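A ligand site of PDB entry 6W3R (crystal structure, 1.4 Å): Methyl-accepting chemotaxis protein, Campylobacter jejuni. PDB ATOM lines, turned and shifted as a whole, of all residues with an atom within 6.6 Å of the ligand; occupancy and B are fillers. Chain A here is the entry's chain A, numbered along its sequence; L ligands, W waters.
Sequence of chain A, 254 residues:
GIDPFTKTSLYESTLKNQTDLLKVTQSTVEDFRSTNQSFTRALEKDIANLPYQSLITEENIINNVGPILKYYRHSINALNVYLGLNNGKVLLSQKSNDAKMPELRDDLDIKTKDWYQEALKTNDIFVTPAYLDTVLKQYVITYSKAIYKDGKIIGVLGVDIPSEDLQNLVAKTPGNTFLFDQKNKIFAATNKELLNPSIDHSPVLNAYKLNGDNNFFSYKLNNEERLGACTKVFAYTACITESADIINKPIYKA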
ATOM      1  N   ASN A  80      -3.244  32.574 -10.402  1.00  0.00           N
ATOM      2  CA  ASN A  80      -4.012  32.198  -9.209  1.00  0.00           C
ATOM      3  C   ASN A  80      -3.599  33.092  -8.050  1.00  0.00           C
ATOM      4  O   ASN A  80      -2.395  33.379  -7.938  1.00  0.00           O
ATOM      5  CB  ASN A  80      -3.767  30.749  -8.737  1.00  0.00           C
ATOM      6  CG  ASN A  80      -4.132  29.717  -9.791  1.00  0.00           C
ATOM      7  OD1 ASN A  80      -5.287  29.599 -10.210  1.00  0.00           O
ATOM      8  ND2 ASN A  80      -3.129  28.933 -10.207  1.00  0.00           N
ATOM      9  N   TYR A  82      -4.686  33.267  -3.777  1.00  0.00           N
ATOM     10  CA  TYR A  82      -5.362  32.375  -2.876  1.00  0.00           C
ATOM     11  C   TYR A  82      -4.959  32.522  -1.439  1.00  0.00           C
ATOM     12  O   TYR A  82      -3.859  32.995  -1.159  1.00  0.00           O
ATOM     13  CB  TYR A  82      -5.180  30.900  -3.342  1.00  0.00           C
ATOM     14  CG  TYR A  82      -3.767  30.506  -3.685  1.00  0.00           C
ATOM     15  CD1 TYR A  82      -3.263  30.739  -4.958  1.00  0.00           C
ATOM     16  CD2 TYR A  82      -2.980  29.834  -2.795  1.00  0.00           C
ATOM     17  CE1 TYR A  82      -1.969  30.325  -5.318  1.00  0.00           C
ATOM     18  CE2 TYR A  82      -1.684  29.443  -3.131  1.00  0.00           C
ATOM     19  CZ  TYR A  82      -1.229  29.593  -4.444  1.00  0.00           C
ATOM     20  OH  TYR A  82       0.032  29.189  -4.781  1.00  0.00           O
ATOM     21  N   VAL A  90      -8.567  26.041   0.952  1.00  0.00           N
ATOM     22  CA  VAL A  90      -7.975  27.218   0.297  1.00  0.00           C
ATOM     23  C   VAL A  90      -9.031  28.004  -0.454  1.00  0.00           C
ATOM     24  O   VAL A  90      -9.832  27.459  -1.245  1.00  0.00           O
ATOM     25  CB  VAL A  90      -6.800  26.834  -0.613  1.00  0.00           C
ATOM     26  CG1 VAL A  90      -7.209  25.837  -1.703  1.00  0.00           C
ATOM     27  CG2 VAL A  90      -6.183  28.062  -1.257  1.00  0.00           C
ATOM     28  N   LEU A  92      -9.662  30.217  -3.371  1.00  0.00           N
ATOM     29  CA  LEU A  92      -8.953  30.302  -4.625  1.00  0.00           C
ATOM     30  C   LEU A  92      -9.618  31.222  -5.608  1.00  0.00           C
ATOM     31  O   LEU A  92     -10.750  30.982  -6.042  1.00  0.00           O
ATOM     32  CB  LEU A  92      -8.869  28.899  -5.229  1.00  0.00           C
ATOM     33  CG  LEU A  92      -8.180  28.771  -6.574  1.00  0.00           C
ATOM     34  CD1 LEU A  92      -6.743  29.268  -6.606  1.00  0.00           C
ATOM     35  CD2 LEU A  92      -8.261  27.335  -7.091  1.00  0.00           C
ATOM     36  N   LEU A 108      -7.127  20.336  -2.551  1.00  0.00           N
ATOM     37  CA  LEU A 108      -5.887  20.725  -3.202  1.00  0.00           C
ATOM     38  C   LEU A 108      -4.660  20.463  -2.336  1.00  0.00           C
ATOM     39  O   LEU A 108      -3.546  20.878  -2.691  1.00  0.00           O
ATOM     40  CB  LEU A 108      -5.980  22.175  -3.659  1.00  0.00           C
ATOM     41  CG  LEU A 108      -6.970  22.434  -4.808  1.00  0.00           C
ATOM     42  CD1 LEU A 108      -7.175  23.920  -5.018  1.00  0.00           C
ATOM     43  CD2 LEU A 108      -6.526  21.796  -6.096  1.00  0.00           C
ATOM     44  N   ASP A 109      -4.820  19.706  -1.247  1.00  0.00           N
ATOM     45  CA  ASP A 109      -3.678  19.139  -0.463  1.00  0.00           C
ATOM     46  C   ASP A 109      -2.637  20.170  -0.076  1.00  0.00           C
ATOM     47  O   ASP A 109      -1.435  19.953  -0.243  1.00  0.00           O
ATOM     48  CB  ASP A 109      -2.969  18.048  -1.258  1.00  0.00           C
ATOM     49  CG  ASP A 109      -3.887  16.919  -1.627  1.00  0.00           C
ATOM     50  OD1 ASP A 109      -4.616  16.440  -0.740  1.00  0.00           O
ATOM     51  OD2 ASP A 109      -3.940  16.579  -2.831  1.00  0.00           O
ATOM     52  N   ILE A 110      -3.094  21.264   0.498  1.00  0.00           N
ATOM     53  CA  ILE A 110      -2.240  22.428   0.584  1.00  0.00           C
ATOM     54  C   ILE A 110      -1.130  22.254   1.593  1.00  0.00           C
ATOM     55  O   ILE A 110      -0.036  22.758   1.389  1.00  0.00           O
ATOM     56  CB  ILE A 110      -3.030  23.725   0.852  1.00  0.00           C
ATOM     57  CG1 ILE A 110      -3.598  23.720   2.273  1.00  0.00           C
ATOM     58  CG2 ILE A 110      -4.052  23.993  -0.274  1.00  0.00           C
ATOM     59  CD1 ILE A 110      -4.320  24.982   2.665  1.00  0.00           C
ATOM     60  N   LYS A 113       2.292  21.213   0.296  1.00  0.00           N
ATOM     61  CA  LYS A 113       2.997  22.072  -0.628  1.00  0.00           C
ATOM     62  C   LYS A 113       4.113  22.899   0.036  1.00  0.00           C
ATOM     63  O   LYS A 113       3.924  23.467   1.097  1.00  0.00           O
ATOM     64  CB  LYS A 113       2.005  23.002  -1.329  1.00  0.00           C
ATOM     65  CG  LYS A 113       0.846  22.296  -2.003  1.00  0.00           C
ATOM     66  CD  LYS A 113       1.282  21.295  -3.056  1.00  0.00           C
ATOM     67  CE  LYS A 113       0.119  20.493  -3.601  1.00  0.00           C
ATOM     68  NZ  LYS A 113      -0.330  21.012  -4.902  1.00  0.00           N
ATOM     69  N   TRP A 115       4.975  25.914  -0.893  1.00  0.00           N
ATOM     70  CA  TRP A 115       4.595  27.305  -0.727  1.00  0.00           C
ATOM     71  C   TRP A 115       3.876  27.528   0.592  1.00  0.00           C
ATOM     72  O   TRP A 115       4.054  28.561   1.239  1.00  0.00           O
ATOM     73  CB  TRP A 115       3.725  27.787  -1.908  1.00  0.00           C
ATOM     74  CG  TRP A 115       2.402  27.119  -2.081  1.00  0.00           C
ATOM     75  CD1 TRP A 115       2.100  26.172  -3.012  1.00  0.00           C
ATOM     76  CD2 TRP A 115       1.199  27.353  -1.338  1.00  0.00           C
ATOM     77  NE1 TRP A 115       0.791  25.819  -2.918  1.00  0.00           N
ATOM     78  CE2 TRP A 115       0.236  26.464  -1.853  1.00  0.00           C
ATOM     79  CE3 TRP A 115       0.824  28.224  -0.330  1.00  0.00           C
ATOM     80  CZ2 TRP A 115      -1.053  26.432  -1.374  1.00  0.00           C
ATOM     81  CZ3 TRP A 115      -0.469  28.188   0.133  1.00  0.00           C
ATOM     82  CH2 TRP A 115      -1.375  27.267  -0.349  1.00  0.00           C
ATOM     83  N   TYR A 131       7.202  25.461 -11.060  1.00  0.00           N
ATOM     84  CA  TYR A 131       6.602  24.127 -10.984  1.00  0.00           C
ATOM     85  C   TYR A 131       5.234  24.143 -11.631  1.00  0.00           C
ATOM     86  O   TYR A 131       4.700  25.192 -11.951  1.00  0.00           O
ATOM     87  CB  TYR A 131       6.465  23.654  -9.525  1.00  0.00           C
ATOM     88  CG  TYR A 131       5.419  24.420  -8.770  1.00  0.00           C
ATOM     89  CD1 TYR A 131       5.676  25.681  -8.250  1.00  0.00           C
ATOM     90  CD2 TYR A 131       4.133  23.926  -8.698  1.00  0.00           C
ATOM     91  CE1 TYR A 131       4.681  26.424  -7.622  1.00  0.00           C
ATOM     92  CE2 TYR A 131       3.125  24.623  -8.037  1.00  0.00           C
ATOM     93  CZ  TYR A 131       3.395  25.886  -7.520  1.00  0.00           C
ATOM     94  OH  TYR A 131       2.406  26.659  -6.939  1.00  0.00           O
ATOM     95  N   LEU A 132       4.726  22.965 -11.905  1.00  0.00           N
ATOM     96  CA  LEU A 132       3.463  22.843 -12.599  1.00  0.00           C
ATOM     97  C   LEU A 132       2.276  23.012 -11.664  1.00  0.00           C
ATOM     98  O   LEU A 132       1.980  22.152 -10.848  1.00  0.00           O
ATOM     99  CB  LEU A 132       3.396  21.499 -13.291  1.00  0.00           C
ATOM    100  CG  LEU A 132       2.212  21.283 -14.251  1.00  0.00           C
ATOM    101  CD1 LEU A 132       2.237  22.214 -15.443  1.00  0.00           C
ATOM    102  CD2 LEU A 132       2.152  19.831 -14.726  1.00  0.00           C
ATOM    103  N   ASP A 133       1.536  24.092 -11.819  1.00  0.00           N
ATOM    104  CA  ASP A 133       0.335  24.314 -11.018  1.00  0.00           C
ATOM    105  C   ASP A 133      -0.663  23.214 -11.310  1.00  0.00           C
ATOM    106  O   ASP A 133      -1.047  23.014 -12.449  1.00  0.00           O
ATOM    107  CB  ASP A 133      -0.253  25.671 -11.360  1.00  0.00           C
ATOM    108  CG  ASP A 133      -1.643  25.834 -10.868  1.00  0.00           C
ATOM    109  OD1 ASP A 133      -1.931  25.555  -9.697  1.00  0.00           O
ATOM    110  OD2 ASP A 133      -2.429  26.353 -11.674  1.00  0.00           O
ATOM    111  N   THR A 134      -1.206  22.668 -10.231  1.00  0.00           N
ATOM    112  CA  THR A 134      -2.254  21.640 -10.274  1.00  0.00           C
ATOM    113  C   THR A 134      -3.601  22.131 -10.840  1.00  0.00           C
ATOM    114  O   THR A 134      -4.269  21.389 -11.551  1.00  0.00           O
ATOM    115  CB  THR A 134      -2.492  21.106  -8.838  1.00  0.00           C
ATOM    116  OG1 THR A 134      -1.334  20.394  -8.391  1.00  0.00           O
ATOM    117  CG2 THR A 134      -3.687  20.165  -8.769  1.00  0.00           C
ATOM    118  N   VAL A 135      -3.935  23.398 -10.627  1.00  0.00           N
ATOM    119  CA  VAL A 135      -5.263  23.873 -11.015  1.00  0.00           C
ATOM    120  C   VAL A 135      -5.382  24.175 -12.513  1.00  0.00           C
ATOM    121  O   VAL A 135      -6.256  23.678 -13.215  1.00  0.00           O
ATOM    122  CB  VAL A 135      -5.692  25.108 -10.167  1.00  0.00           C
ATOM    123  CG1 VAL A 135      -6.964  25.723 -10.710  1.00  0.00           C
ATOM    124  CG2 VAL A 135      -5.960  24.670  -8.732  1.00  0.00           C
ATOM    125  N   VAL A 140       4.424  27.827 -12.993  1.00  0.00           N
ATOM    126  CA  VAL A 140       4.343  29.068 -12.223  1.00  0.00           C
ATOM    127  C   VAL A 140       5.494  29.217 -11.261  1.00  0.00           C
ATOM    128  O   VAL A 140       6.125  28.240 -10.842  1.00  0.00           O
ATOM    129  CB  VAL A 140       3.014  29.138 -11.438  1.00  0.00           C
ATOM    130  CG1 VAL A 140       1.833  29.094 -12.397  1.00  0.00           C
ATOM    131  CG2 VAL A 140       2.941  28.080 -10.367  1.00  0.00           C
ATOM    132  N   THR A 142       5.549  30.787  -7.499  1.00  0.00           N
ATOM    133  CA  THR A 142       4.619  31.142  -6.432  1.00  0.00           C
ATOM    134  C   THR A 142       5.327  32.000  -5.413  1.00  0.00           C
ATOM    135  O   THR A 142       6.423  31.648  -4.958  1.00  0.00           O
ATOM    136  CB  THR A 142       3.973  29.869  -5.813  1.00  0.00           C
ATOM    137  OG1 THR A 142       3.196  29.187  -6.822  1.00  0.00           O
ATOM    138  CG2 THR A 142       3.095  30.215  -4.609  1.00  0.00           C
ATOM    139  N   ASP A 160       0.417  32.998  -7.838  1.00  0.00           N
ATOM    140  CA  ASP A 160       1.081  32.263  -8.878  1.00  0.00           C
ATOM    141  C   ASP A 160       1.208  33.148 -10.104  1.00  0.00           C
ATOM    142  O   ASP A 160       0.181  33.588 -10.690  1.00  0.00           O
ATOM    143  CB  ASP A 160       0.209  31.065  -9.311  1.00  0.00           C
ATOM    144  CG  ASP A 160       0.088  29.982  -8.265  1.00  0.00           C
ATOM    145  OD1 ASP A 160       0.773  29.996  -7.215  1.00  0.00           O
ATOM    146  OD2 ASP A 160      -0.696  29.030  -8.467  1.00  0.00           O
HETATM  147  N1  LIG L   1      -0.447  26.438  -7.644  1.00  0.00           N
HETATM  148  C1  LIG L   1      -0.817  25.943  -6.293  1.00  0.00           C
HETATM  149  C2  LIG L   1      -2.324  25.876  -5.994  1.00  0.00           C
HETATM  150  C3  LIG L   1      -2.937  27.100  -6.680  1.00  0.00           C
HETATM  151  C4  LIG L   1      -2.989  24.599  -6.501  1.00  0.00           C
HETATM  152  C5  LIG L   1      -2.488  25.923  -4.437  1.00  0.00           C
HETATM  153  C6  LIG L   1      -3.926  26.141  -3.925  1.00  0.00           C
HETATM  154  C7  LIG L   1      -0.292  24.513  -6.155  1.00  0.00           C
HETATM  155  O1  LIG L   1      -0.061  23.879  -7.208  1.00  0.00           O
HETATM  156  O2  LIG L   1      -0.053  24.044  -5.005  1.00  0.00           O
HETATM  157  O   HOH W   1       1.340  21.577  -7.204  1.00  0.00           O
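O2 of the ligand is in salt-bridge range of NZ of Lys 113, 3.0 Å away. The side-chain carboxylate (OD2) of Asp 160 lies within salt-bridge range of a nitrogen (N1) of the ligand, at 2.7 Å. The backbone NH of Thr 134 is in hydrogen-bond range of an oxygen (O1) of the ligand (3.5 Å). NE1 of Trp 115 is in hydrogen-bond range of O2 of the ligand (2.9 Å). The side-chain carboxylate (OD1) of Asp 133 is in salt-bridge range of a nitrogen (N1) of the ligand (2.7 Å). The side-chain hydroxyl (OH) of Tyr 131 is in hydrogen-bond range of a nitrogen (N1) of the ligand, at 2.9 Å.
OD2 of Asp 133 is in hydrogen-bond range of ND2 of Asn 80 (3.0 Å). The backbone NH (N) of Val 140 lies within hydrogen-bond range of the backbone carbonyl oxygen (O) of Tyr 131 (2.8 Å). The side-chain hydroxyl of Thr 142 sits at hydrogen-bond distance from the side-chain hydroxyl of Tyr 131 (2.7 Å). OD1 of Asp 160 lies within hydrogen-bond range of OH of Tyr 82. The backbone NH (N) of Asp 160 is in hydrogen-bond range of the backbone carbonyl oxygen (O) of Asn 80 (2.8 Å). OG1 of Thr 142 lies within hydrogen-bond range of OD1 of Asp 160. The side-chain carboxylate of Asp 133 sits at hydrogen-bond distance from the backbone NH of Val 135.
Residues that only touch the ligand: Asn 80 (3.98 Å), Tyr 82 (3.6 Å), Val 90 (3.98 Å) and Val 135 (3.7 Å). Hydrophobic or aromatic side chains within 4 Å of the ligand: Tyr 82, Val 90, Trp 115, Tyr 131 and Val 135. Ten residues have an atom within 4 Å of the ligand: Asn 80, Tyr 82, Val 90, Lys 113, Trp 115, Tyr 131, Asp 133, Thr 134, Val 135 and Asp 160. The nearest printed residue that does not touch the ligand is Leu 108 (4.1 Å).
Water W1 lies within hydrogen-bond range of an oxygen (O1) of the ligand, the side-chain amino group of Lys 113 and the side-chain hydroxyl of Thr 134.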
